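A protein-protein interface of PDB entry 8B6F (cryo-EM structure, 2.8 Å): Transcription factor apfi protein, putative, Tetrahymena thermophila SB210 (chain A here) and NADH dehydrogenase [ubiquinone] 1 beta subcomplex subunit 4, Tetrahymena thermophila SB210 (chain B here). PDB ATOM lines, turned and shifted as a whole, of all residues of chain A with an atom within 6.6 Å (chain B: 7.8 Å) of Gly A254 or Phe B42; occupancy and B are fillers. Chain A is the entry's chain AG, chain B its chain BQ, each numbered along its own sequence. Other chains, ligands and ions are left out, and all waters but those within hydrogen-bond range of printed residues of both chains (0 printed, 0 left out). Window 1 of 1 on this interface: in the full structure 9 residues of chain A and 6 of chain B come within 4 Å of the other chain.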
ATOM      1  N   LYS A 249      23.923  17.544  23.927  1.00  0.00           N
ATOM      2  CA  LYS A 249      22.845  17.399  24.898  1.00  0.00           C
ATOM      3  C   LYS A 249      22.538  15.928  25.157  1.00  0.00           C
ATOM      4  O   LYS A 249      22.283  15.531  26.298  1.00  0.00           O
ATOM      5  CB  LYS A 249      21.596  18.139  24.416  1.00  0.00           C
ATOM      6  CG  LYS A 249      21.580  19.622  24.771  1.00  0.00           C
ATOM      7  CD  LYS A 249      22.699  20.377  24.068  1.00  0.00           C
ATOM      8  CE  LYS A 249      22.726  21.842  24.465  1.00  0.00           C
ATOM      9  NZ  LYS A 249      23.881  22.561  23.854  1.00  0.00           N
ATOM     10  N   MET A 250      22.570  15.103  24.108  1.00  0.00           N
ATOM     11  CA  MET A 250      22.283  13.680  24.277  1.00  0.00           C
ATOM     12  C   MET A 250      23.326  12.995  25.150  1.00  0.00           C
ATOM     13  O   MET A 250      22.979  12.184  26.016  1.00  0.00           O
ATOM     14  CB  MET A 250      22.208  12.997  22.913  1.00  0.00           C
ATOM     15  CG  MET A 250      20.971  13.352  22.112  1.00  0.00           C
ATOM     16  SD  MET A 250      20.992  12.620  20.470  1.00  0.00           S
ATOM     17  CE  MET A 250      19.543  13.387  19.761  1.00  0.00           C
ATOM     18  N   ARG A 251      24.607  13.298  24.943  1.00  0.00           N
ATOM     19  CA  ARG A 251      25.636  12.680  25.773  1.00  0.00           C
ATOM     20  C   ARG A 251      25.540  13.166  27.213  1.00  0.00           C
ATOM     21  O   ARG A 251      25.797  12.401  28.150  1.00  0.00           O
ATOM     22  CB  ARG A 251      27.027  12.952  25.196  1.00  0.00           C
ATOM     23  CG  ARG A 251      27.480  14.400  25.278  1.00  0.00           C
ATOM     24  CD  ARG A 251      28.957  14.540  24.955  1.00  0.00           C
ATOM     25  NE  ARG A 251      29.399  15.924  25.059  1.00  0.00           N
ATOM     26  CZ  ARG A 251      29.715  16.532  26.194  1.00  0.00           C
ATOM     27  NH1 ARG A 251      29.650  15.904  27.356  1.00  0.00           N
ATOM     28  NH2 ARG A 251      30.104  17.803  26.161  1.00  0.00           N
ATOM     29  N   ASP A 252      25.174  14.433  27.414  1.00  0.00           N
ATOM     30  CA  ASP A 252      24.953  14.919  28.771  1.00  0.00           C
ATOM     31  C   ASP A 252      23.804  14.171  29.435  1.00  0.00           C
ATOM     32  O   ASP A 252      23.876  13.834  30.621  1.00  0.00           O
ATOM     33  CB  ASP A 252      24.673  16.422  28.750  1.00  0.00           C
ATOM     34  CG  ASP A 252      25.896  17.238  28.378  1.00  0.00           C
ATOM     35  OD1 ASP A 252      27.020  16.816  28.715  1.00  0.00           O
ATOM     36  OD2 ASP A 252      25.733  18.303  27.745  1.00  0.00           O
ATOM     37  N   LEU A 253      22.730  13.910  28.686  1.00  0.00           N
ATOM     38  CA  LEU A 253      21.605  13.168  29.242  1.00  0.00           C
ATOM     39  C   LEU A 253      21.952  11.703  29.467  1.00  0.00           C
ATOM     40  O   LEU A 253      21.365  11.058  30.342  1.00  0.00           O
ATOM     41  CB  LEU A 253      20.390  13.287  28.323  1.00  0.00           C
ATOM     42  CG  LEU A 253      19.435  14.446  28.616  1.00  0.00           C
ATOM     43  CD1 LEU A 253      20.142  15.793  28.597  1.00  0.00           C
ATOM     44  CD2 LEU A 253      18.293  14.435  27.615  1.00  0.00           C
ATOM     45  N   GLY A 254      22.882  11.162  28.693  1.00  0.00           N
ATOM     46  CA  GLY A 254      23.309   9.791  28.832  1.00  0.00           C
ATOM     47  C   GLY A 254      22.884   8.846  27.724  1.00  0.00           C
ATOM     48  O   GLY A 254      22.854   7.632  27.957  1.00  0.00           O
ATOM     49  N   PHE A 255      22.555   9.353  26.539  1.00  0.00           N
ATOM     50  CA  PHE A 255      22.152   8.484  25.448  1.00  0.00           C
ATOM     51  C   PHE A 255      23.353   7.706  24.915  1.00  0.00           C
ATOM     52  O   PHE A 255      24.503   8.100  25.123  1.00  0.00           O
ATOM     53  CB  PHE A 255      21.527   9.296  24.316  1.00  0.00           C
ATOM     54  CG  PHE A 255      20.185   9.892  24.650  1.00  0.00           C
ATOM     55  CD1 PHE A 255      19.675   9.842  25.938  1.00  0.00           C
ATOM     56  CD2 PHE A 255      19.425  10.489  23.660  1.00  0.00           C
ATOM     57  CE1 PHE A 255      18.442  10.389  26.232  1.00  0.00           C
ATOM     58  CE2 PHE A 255      18.193  11.038  23.947  1.00  0.00           C
ATOM     59  CZ  PHE A 255      17.700  10.987  25.234  1.00  0.00           C
ATOM     60  N   PRO A 256      23.113   6.588  24.232  1.00  0.00           N
ATOM     61  CA  PRO A 256      24.226   5.862  23.609  1.00  0.00           C
ATOM     62  C   PRO A 256      24.937   6.732  22.585  1.00  0.00           C
ATOM     63  O   PRO A 256      24.307   7.483  21.840  1.00  0.00           O
ATOM     64  CB  PRO A 256      23.544   4.657  22.949  1.00  0.00           C
ATOM     65  CG  PRO A 256      22.229   4.528  23.633  1.00  0.00           C
ATOM     66  CD  PRO A 256      21.823   5.914  24.009  1.00  0.00           C
ATOM     67  N   MET A 257      26.266   6.609  22.539  1.00  0.00           N
ATOM     68  CA  MET A 257      27.093   7.386  21.622  1.00  0.00           C
ATOM     69  C   MET A 257      27.949   6.498  20.724  1.00  0.00           C
ATOM     70  O   MET A 257      28.898   6.985  20.102  1.00  0.00           O
ATOM     71  CB  MET A 257      27.983   8.353  22.404  1.00  0.00           C
ATOM     72  CG  MET A 257      27.224   9.414  23.196  1.00  0.00           C
ATOM     73  SD  MET A 257      26.662  10.822  22.212  1.00  0.00           S
ATOM     74  CE  MET A 257      25.033  10.301  21.687  1.00  0.00           C
ATOM     75  N   GLU A 258      27.637   5.207  20.642  1.00  0.00           N
ATOM     76  CA  GLU A 258      28.394   4.278  19.818  1.00  0.00           C
ATOM     77  C   GLU A 258      27.443   3.269  19.192  1.00  0.00           C
ATOM     78  O   GLU A 258      26.384   2.966  19.744  1.00  0.00           O
ATOM     79  CB  GLU A 258      29.471   3.556  20.636  1.00  0.00           C
ATOM     80  CG  GLU A 258      30.550   4.484  21.168  1.00  0.00           C
ATOM     81  CD  GLU A 258      31.558   3.769  22.044  1.00  0.00           C
ATOM     82  OE1 GLU A 258      31.271   2.633  22.475  1.00  0.00           O
ATOM     83  OE2 GLU A 258      32.636   4.342  22.303  1.00  0.00           O
ATOM     84  N   GLU A 261      26.513   0.366  21.226  1.00  0.00           N
ATOM     85  CA  GLU A 261      25.656   0.796  22.319  1.00  0.00           C
ATOM     86  C   GLU A 261      24.272   1.227  21.856  1.00  0.00           C
ATOM     87  O   GLU A 261      23.397   1.449  22.698  1.00  0.00           O
ATOM     88  CB  GLU A 261      26.312   1.953  23.077  1.00  0.00           C
ATOM     89  CG  GLU A 261      27.627   1.584  23.740  1.00  0.00           C
ATOM     90  CD  GLU A 261      28.303   2.772  24.388  1.00  0.00           C
ATOM     91  OE1 GLU A 261      27.925   3.917  24.069  1.00  0.00           O
ATOM     92  OE2 GLU A 261      29.209   2.560  25.219  1.00  0.00           O
ATOM     93  N   GLU A 262      24.053   1.358  20.545  1.00  0.00           N
ATOM     94  CA  GLU A 262      22.736   1.731  20.049  1.00  0.00           C
ATOM     95  C   GLU A 262      21.675   0.697  20.395  1.00  0.00           C
ATOM     96  O   GLU A 262      20.483   1.019  20.376  1.00  0.00           O
ATOM     97  CB  GLU A 262      22.774   1.924  18.531  1.00  0.00           C
ATOM     98  CG  GLU A 262      23.598   3.111  18.066  1.00  0.00           C
ATOM     99  CD  GLU A 262      23.065   4.432  18.578  1.00  0.00           C
ATOM    100  OE1 GLU A 262      21.916   4.460  19.064  1.00  0.00           O
ATOM    101  OE2 GLU A 262      23.797   5.441  18.496  1.00  0.00           O
ATOM    102  N   TYR A 264      21.067  -0.649  23.256  1.00  0.00           N
ATOM    103  CA  TYR A 264      20.527  -0.422  24.589  1.00  0.00           C
ATOM    104  C   TYR A 264      19.939   0.979  24.720  1.00  0.00           C
ATOM    105  O   TYR A 264      19.950   1.568  25.801  1.00  0.00           O
ATOM    106  CB  TYR A 264      21.607  -0.649  25.647  1.00  0.00           C
ATOM    107  CG  TYR A 264      22.132  -2.065  25.670  1.00  0.00           C
ATOM    108  CD1 TYR A 264      21.412  -3.083  26.281  1.00  0.00           C
ATOM    109  CD2 TYR A 264      23.348  -2.382  25.082  1.00  0.00           C
ATOM    110  CE1 TYR A 264      21.886  -4.379  26.301  1.00  0.00           C
ATOM    111  CE2 TYR A 264      23.832  -3.675  25.098  1.00  0.00           C
ATOM    112  CZ  TYR A 264      23.097  -4.669  25.710  1.00  0.00           C
ATOM    113  OH  TYR A 264      23.576  -5.958  25.729  1.00  0.00           O
ATOM    114  N   ILE A 265      19.428   1.522  23.614  1.00  0.00           N
ATOM    115  CA  ILE A 265      18.877   2.875  23.632  1.00  0.00           C
ATOM    116  C   ILE A 265      17.663   2.951  24.548  1.00  0.00           C
ATOM    117  O   ILE A 265      17.507   3.909  25.314  1.00  0.00           O
ATOM    118  CB  ILE A 265      18.543   3.330  22.198  1.00  0.00           C
ATOM    119  CG1 ILE A 265      18.045   4.780  22.207  1.00  0.00           C
ATOM    120  CG2 ILE A 265      17.512   2.398  21.556  1.00  0.00           C
ATOM    121  CD1 ILE A 265      17.770   5.353  20.829  1.00  0.00           C
ATOM    122  N   GLN A 267      16.928   1.573  27.222  1.00  0.00           N
ATOM    123  CA  GLN A 267      17.254   1.649  28.640  1.00  0.00           C
ATOM    124  C   GLN A 267      17.630   3.053  29.087  1.00  0.00           C
ATOM    125  O   GLN A 267      17.657   3.316  30.292  1.00  0.00           O
ATOM    126  CB  GLN A 267      18.398   0.695  28.968  1.00  0.00           C
ATOM    127  CG  GLN A 267      17.947  -0.665  29.437  1.00  0.00           C
ATOM    128  CD  GLN A 267      17.216  -1.446  28.371  1.00  0.00           C
ATOM    129  OE1 GLN A 267      17.619  -1.459  27.211  1.00  0.00           O
ATOM    130  NE2 GLN A 267      16.132  -2.103  28.761  1.00  0.00           N
ATOM    131  N   ARG A 268      17.923   3.957  28.152  1.00  0.00           N
ATOM    132  CA  ARG A 268      18.369   5.298  28.491  1.00  0.00           C
ATOM    133  C   ARG A 268      17.411   6.398  28.066  1.00  0.00           C
ATOM    134  O   ARG A 268      17.548   7.526  28.551  1.00  0.00           O
ATOM    135  CB  ARG A 268      19.740   5.581  27.855  1.00  0.00           C
ATOM    136  CG  ARG A 268      20.920   5.133  28.701  1.00  0.00           C
ATOM    137  CD  ARG A 268      21.063   5.988  29.949  1.00  0.00           C
ATOM    138  NE  ARG A 268      22.389   5.871  30.542  1.00  0.00           N
ATOM    139  CZ  ARG A 268      22.734   4.970  31.452  1.00  0.00           C
ATOM    140  NH1 ARG A 268      21.869   4.078  31.907  1.00  0.00           N
ATOM    141  NH2 ARG A 268      23.980   4.963  31.916  1.00  0.00           N
ATOM    142  N   ARG A 272      13.758   4.624  31.796  1.00  0.00           N
ATOM    143  CA  ARG A 272      13.874   5.418  33.013  1.00  0.00           C
ATOM    144  C   ARG A 272      12.557   6.117  33.320  1.00  0.00           C
ATOM    145  O   ARG A 272      11.975   6.784  32.461  1.00  0.00           O
ATOM    146  CB  ARG A 272      14.998   6.444  32.875  1.00  0.00           C
ATOM    147  CG  ARG A 272      16.385   5.850  33.039  1.00  0.00           C
ATOM    148  CD  ARG A 272      17.458   6.925  33.088  1.00  0.00           C
ATOM    149  NE  ARG A 272      17.700   7.519  31.779  1.00  0.00           N
ATOM    150  CZ  ARG A 272      18.612   8.451  31.538  1.00  0.00           C
ATOM    151  NH1 ARG A 272      19.382   8.932  32.499  1.00  0.00           N
ATOM    152  NH2 ARG A 272      18.757   8.910  30.298  1.00  0.00           N
ATOM    153  N   GLN B  34      24.529  13.074  37.357  1.00  0.00           N
ATOM    154  CA  GLN B  34      23.442  12.123  37.156  1.00  0.00           C
ATOM    155  C   GLN B  34      23.946  10.824  36.547  1.00  0.00           C
ATOM    156  O   GLN B  34      23.369   9.758  36.794  1.00  0.00           O
ATOM    157  CB  GLN B  34      22.361  12.739  36.266  1.00  0.00           C
ATOM    158  CG  GLN B  34      21.679  13.965  36.864  1.00  0.00           C
ATOM    159  CD  GLN B  34      20.971  13.670  38.177  1.00  0.00           C
ATOM    160  OE1 GLN B  34      21.014  14.473  39.109  1.00  0.00           O
ATOM    161  NE2 GLN B  34      20.309  12.519  38.253  1.00  0.00           N
ATOM    162  N   VAL B  35      25.011  10.890  35.747  1.00  0.00           N
ATOM    163  CA  VAL B  35      25.544   9.686  35.117  1.00  0.00           C
ATOM    164  C   VAL B  35      26.044   8.708  36.171  1.00  0.00           C
ATOM    165  O   VAL B  35      25.837   7.493  36.059  1.00  0.00           O
ATOM    166  CB  VAL B  35      26.651  10.055  34.110  1.00  0.00           C
ATOM    167  CG1 VAL B  35      27.824  10.740  34.806  1.00  0.00           C
ATOM    168  CG2 VAL B  35      27.122   8.816  33.362  1.00  0.00           C
ATOM    169  N   GLU B  38      23.659   6.275  37.716  1.00  0.00           N
ATOM    170  CA  GLU B  38      23.038   5.300  36.838  1.00  0.00           C
ATOM    171  C   GLU B  38      23.554   3.894  37.148  1.00  0.00           C
ATOM    172  O   GLU B  38      24.671   3.728  37.641  1.00  0.00           O
ATOM    173  CB  GLU B  38      23.321   5.642  35.379  1.00  0.00           C
ATOM    174  CG  GLU B  38      22.877   7.037  34.975  1.00  0.00           C
ATOM    175  CD  GLU B  38      21.386   7.253  35.151  1.00  0.00           C
ATOM    176  OE1 GLU B  38      20.645   6.254  35.254  1.00  0.00           O
ATOM    177  OE2 GLU B  38      20.955   8.425  35.187  1.00  0.00           O
ATOM    178  N   PHE B  40      24.240   1.248  34.998  1.00  0.00           N
ATOM    179  CA  PHE B  40      25.244   0.780  34.054  1.00  0.00           C
ATOM    180  C   PHE B  40      25.811   1.960  33.276  1.00  0.00           C
ATOM    181  O   PHE B  40      25.152   2.989  33.108  1.00  0.00           O
ATOM    182  CB  PHE B  40      24.662  -0.265  33.089  1.00  0.00           C
ATOM    183  CG  PHE B  40      23.608   0.275  32.170  1.00  0.00           C
ATOM    184  CD1 PHE B  40      22.296   0.393  32.595  1.00  0.00           C
ATOM    185  CD2 PHE B  40      23.924   0.647  30.875  1.00  0.00           C
ATOM    186  CE1 PHE B  40      21.320   0.883  31.750  1.00  0.00           C
ATOM    187  CE2 PHE B  40      22.955   1.139  30.025  1.00  0.00           C
ATOM    188  CZ  PHE B  40      21.650   1.255  30.463  1.00  0.00           C
ATOM    189  N   LYS B  41      27.047   1.799  32.805  1.00  0.00           N
ATOM    190  CA  LYS B  41      27.792   2.865  32.155  1.00  0.00           C
ATOM    191  C   LYS B  41      28.111   2.495  30.714  1.00  0.00           C
ATOM    192  O   LYS B  41      28.320   1.324  30.387  1.00  0.00           O
ATOM    193  CB  LYS B  41      29.103   3.155  32.896  1.00  0.00           C
ATOM    194  CG  LYS B  41      28.938   3.488  34.369  1.00  0.00           C
ATOM    195  CD  LYS B  41      28.268   4.834  34.560  1.00  0.00           C
ATOM    196  CE  LYS B  41      28.206   5.212  36.028  1.00  0.00           C
ATOM    197  NZ  LYS B  41      27.389   4.252  36.821  1.00  0.00           N
ATOM    198  N   PHE B  42      28.150   3.510  29.853  1.00  0.00           N
ATOM    199  CA  PHE B  42      28.612   3.357  28.484  1.00  0.00           C
ATOM    200  C   PHE B  42      30.108   3.666  28.407  1.00  0.00           C
ATOM    201  O   PHE B  42      30.768   3.917  29.416  1.00  0.00           O
ATOM    202  CB  PHE B  42      27.807   4.260  27.548  1.00  0.00           C
ATOM    203  CG  PHE B  42      26.397   3.794  27.304  1.00  0.00           C
ATOM    204  CD1 PHE B  42      26.105   2.447  27.147  1.00  0.00           C
ATOM    205  CD2 PHE B  42      25.362   4.709  27.221  1.00  0.00           C
ATOM    206  CE1 PHE B  42      24.810   2.025  26.916  1.00  0.00           C
ATOM    207  CE2 PHE B  42      24.065   4.293  26.990  1.00  0.00           C
ATOM    208  CZ  PHE B  42      23.789   2.950  26.839  1.00  0.00           C
ATOM    209  N   ASN B  43      30.653   3.664  27.188  1.00  0.00           N
ATOM    210  CA  ASN B  43      32.090   3.868  27.028  1.00  0.00           C
ATOM    211  C   ASN B  43      32.505   5.267  27.468  1.00  0.00           C
ATOM    212  O   ASN B  43      33.457   5.427  28.240  1.00  0.00           O
ATOM    213  CB  ASN B  43      32.498   3.624  25.576  1.00  0.00           C
ATOM    214  CG  ASN B  43      32.516   2.153  25.216  1.00  0.00           C
ATOM    215  OD1 ASN B  43      33.493   1.451  25.474  1.00  0.00           O
ATOM    216  ND2 ASN B  43      31.435   1.678  24.612  1.00  0.00           N
ATOM    217  N   HIS B  44      31.807   6.296  26.985  1.00  0.00           N
ATOM    218  CA  HIS B  44      32.193   7.660  27.332  1.00  0.00           C
ATOM    219  C   HIS B  44      31.967   7.933  28.813  1.00  0.00           C
ATOM    220  O   HIS B  44      32.735   8.671  29.439  1.00  0.00           O
ATOM    221  CB  HIS B  44      31.428   8.665  26.470  1.00  0.00           C
ATOM    222  CG  HIS B  44      29.943   8.605  26.639  1.00  0.00           C
ATOM    223  ND1 HIS B  44      29.155   7.688  25.976  1.00  0.00           N
ATOM    224  CD2 HIS B  44      29.099   9.359  27.380  1.00  0.00           C
ATOM    225  CE1 HIS B  44      27.890   7.875  26.311  1.00  0.00           C
ATOM    226  NE2 HIS B  44      27.828   8.883  27.161  1.00  0.00           N
ATOM    227  N   GLU B  45      30.912   7.353  29.386  1.00  0.00           N
ATOM    228  CA  GLU B  45      30.673   7.501  30.817  1.00  0.00           C
ATOM    229  C   GLU B  45      31.756   6.800  31.628  1.00  0.00           C
ATOM    230  O   GLU B  45      32.214   7.325  32.647  1.00  0.00           O
ATOM    231  CB  GLU B  45      29.289   6.958  31.168  1.00  0.00           C
ATOM    232  CG  GLU B  45      28.168   7.590  30.350  1.00  0.00           C
ATOM    233  CD  GLU B  45      26.817   6.965  30.625  1.00  0.00           C
ATOM    234  OE1 GLU B  45      26.778   5.806  31.085  1.00  0.00           O
ATOM    235  OE2 GLU B  45      25.790   7.632  30.382  1.00  0.00           O
ATOM    236  N   ARG B  46      32.177   5.612  31.188  1.00  0.00           N
ATOM    237  CA  ARG B  46      33.238   4.894  31.888  1.00  0.00           C
ATOM    238  C   ARG B  46      34.560   5.644  31.814  1.00  0.00           C
ATOM    239  O   ARG B  46      35.327   5.655  32.782  1.00  0.00           O
ATOM    240  CB  ARG B  46      33.406   3.495  31.300  1.00  0.00           C
ATOM    241  CG  ARG B  46      32.354   2.500  31.732  1.00  0.00           C
ATOM    242  CD  ARG B  46      32.592   1.155  31.069  1.00  0.00           C
ATOM    243  NE  ARG B  46      31.668   0.136  31.547  1.00  0.00           N
ATOM    244  CZ  ARG B  46      31.640  -1.113  31.107  1.00  0.00           C
ATOM    245  NH1 ARG B  46      32.470  -1.533  30.166  1.00  0.00           N
ATOM    246  NH2 ARG B  46      30.757  -1.964  31.621  1.00  0.00           N
ATOM    247  N   ASP B  47      34.838   6.285  30.678  1.00  0.00           N
ATOM    248  CA  ASP B  47      36.131   6.938  30.501  1.00  0.00           C
ATOM    249  C   ASP B  47      36.347   8.023  31.545  1.00  0.00           C
ATOM    250  O   ASP B  47      37.434   8.130  32.123  1.00  0.00           O
ATOM    251  CB  ASP B  47      36.229   7.519  29.091  1.00  0.00           C
ATOM    252  CG  ASP B  47      37.626   8.006  28.757  1.00  0.00           C
ATOM    253  OD1 ASP B  47      38.522   7.884  29.620  1.00  0.00           O
ATOM    254  OD2 ASP B  47      37.828   8.506  27.632  1.00  0.00           O
ATOM    255  N   GLN B  48      35.328   8.846  31.794  1.00  0.00           N
ATOM    256  CA  GLN B  48      35.470   9.916  32.775  1.00  0.00           C
ATOM    257  C   GLN B  48      35.767   9.358  34.161  1.00  0.00           C
ATOM    258  O   GLN B  48      36.622   9.886  34.880  1.00  0.00           O
ATOM    259  CB  GLN B  48      34.202  10.767  32.802  1.00  0.00           C
ATOM    260  CG  GLN B  48      33.876  11.419  31.467  1.00  0.00           C
ATOM    261  CD  GLN B  48      32.530  12.111  31.472  1.00  0.00           C
ATOM    262  OE1 GLN B  48      31.712  11.896  32.364  1.00  0.00           O
ATOM    263  NE2 GLN B  48      32.297  12.956  30.474  1.00  0.00           N
ATOM    264  N   ILE B  50      37.099   6.357  34.982  1.00  0.00           N
ATOM    265  CA  ILE B  50      38.339   5.593  35.073  1.00  0.00           C
ATOM    266  C   ILE B  50      39.517   6.438  34.612  1.00  0.00           C
ATOM    267  O   ILE B  50      40.628   5.924  34.447  1.00  0.00           O
ATOM    268  CB  ILE B  50      38.261   4.290  34.254  1.00  0.00           C
ATOM    269  CG1 ILE B  50      38.336   4.597  32.752  1.00  0.00           C
ATOM    270  CG2 ILE B  50      36.989   3.525  34.612  1.00  0.00           C
ATOM    271  CD1 ILE B  50      38.107   3.402  31.847  1.00  0.00           C
ATOM    272  N   MET B  55      41.122  -0.147  32.419  1.00  0.00           N
ATOM    273  CA  MET B  55      40.022  -1.071  32.676  1.00  0.00           C
ATOM    274  C   MET B  55      40.512  -2.319  33.396  1.00  0.00           C
ATOM    275  O   MET B  55      39.861  -2.801  34.329  1.00  0.00           O
ATOM    276  CB  MET B  55      39.336  -1.451  31.365  1.00  0.00           C
ATOM    277  CG  MET B  55      38.544  -0.323  30.723  1.00  0.00           C
ATOM    278  SD  MET B  55      37.131   0.216  31.709  1.00  0.00           S
ATOM    279  CE  MET B  55      36.114  -1.258  31.705  1.00  0.00           C
ATOM    280  N   TYR B  59      38.683  -2.821  36.950  1.00  0.00           N
ATOM    281  CA  TYR B  59      37.740  -3.931  36.944  1.00  0.00           C
ATOM    282  C   TYR B  59      38.415  -5.294  36.925  1.00  0.00           C
ATOM    283  O   TYR B  59      37.730  -6.306  37.115  1.00  0.00           O
ATOM    284  CB  TYR B  59      36.808  -3.819  35.736  1.00  0.00           C
ATOM    285  CG  TYR B  59      36.015  -2.535  35.687  1.00  0.00           C
ATOM    286  CD1 TYR B  59      36.540  -1.394  35.095  1.00  0.00           C
ATOM    287  CD2 TYR B  59      34.737  -2.468  36.221  1.00  0.00           C
ATOM    288  CE1 TYR B  59      35.815  -0.220  35.044  1.00  0.00           C
ATOM    289  CE2 TYR B  59      34.004  -1.300  36.176  1.00  0.00           C
ATOM    290  CZ  TYR B  59      34.548  -0.180  35.585  1.00  0.00           C
ATOM    291  OH  TYR B  59      33.820   0.985  35.538  1.00  0.00           O
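The side-chain carboxylate (OE2) of Glu A261 is in hydrogen-bond range of the side-chain amide nitrogen (ND2) of Asn B43.
The side-chain carboxylate of Glu B38 is in salt-bridge range of the guanidinium group of Arg A272, at 3.2 Å.
NH2 of Arg A268 lies within salt-bridge range of OE1 of Glu B45, at 3.0 Å.
The guanidinium group (NH2) of Arg A268 sits at hydrogen-bond distance from the backbone carbonyl oxygen (O) of Phe B40 (2.6 Å).
ND2 of Asn B43 lies close to OE1 of Glu A258 (2.3 Å).
NE of Arg A268 sits close to O of Gly A254 (3.2 Å).
N of Phe A255 sits at hydrogen-bond distance from O of Met A250, at 2.9 Å.
NZ of Lys B41 sits at hydrogen-bond distance from O of Glu B38, at 2.9 Å.
The backbone NH (N) of Phe B42 lies within hydrogen-bond range of the side-chain carboxylate (OE1) of Glu B45, at 2.9 Å.
The backbone carbonyl oxygen (O) of Arg A268 sits at hydrogen-bond distance from the guanidinium group (NH2) of Arg A272 (2.5 Å).
The backbone carbonyl oxygen (O) of Leu A253 is in hydrogen-bond range of the guanidinium group (NH2) of Arg A272 (3.4 Å).
Gly A254 touches Phe B42.
Glu B45 touches Gly A254 (OE2 to CA, 3.6 Å).
O of Phe A255 touches CE1 of His B44, 3.6 Å away.
Pro A256 touches Phe B42 (N to CE2, 3.7 Å).
Met A257 touches His B44 (CG to CE1, 3.5 Å).
Glu A261 touches Phe B42 (OE2 to CB, 3.2 Å).
CB of Gln A267 touches CZ of Phe B40, at 3.6 Å.
Arg A268 touches Glu B38 (NH2 to CB, 3.6 Å).
CG of Arg A268 touches CE2 of Phe B42, 3.7 Å away.
Of chain B, only Phe B42 and Glu B45 come within 4 Å of Gly A254.
Of the printed residues of chain B, Pro A256 touches Phe B42 (3.7 Å).
Of chain A, only Gly A254 (3.7 Å), Pro A256 (3.7 Å), Glu A261 (3.2 Å) and Arg A268 (3.7 Å) come within 4 Å of Phe B42.
Printed residues of chain A within 4 Å of Asn B43: Glu A258 and Glu A261.
Of the printed residues of chain A, Glu B45 touches Gly A254 and Arg A268.
The nearest residue of chain B that does not touch Gly A254 is His B44 (4.9 Å).
The nearest printed residue of chain B that does not touch Met A257 is Phe B42 (5.1 Å).
Of the 17 printed residues of chain A, 9 touch a printed residue of chain B.
Hydrophobic or aromatic side chains of chain A within 4 Å of the printed part of chain B: Pro A256 and Met A257.
Of the 15 printed residues of chain B, 6 touch a printed residue of chain A.
Printed residues of chain B that touch a printed residue of chain A: Glu B38, Phe B40, Phe B42, Asn B43, His B44 and Glu B45.
Along chain B the printed residues that touch a printed residue of chain A span positions 38 to 45.
Among the printed residues, 14 pairs touch across the chains.
Among the printed residues, Asp or Glu carboxylates within 4 Å of a Lys or Arg side-chain nitrogen of the other chain: Arg A268 with Glu B45 (3.0 Å) and Arg A272 with Glu B38 (3.2 Å).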
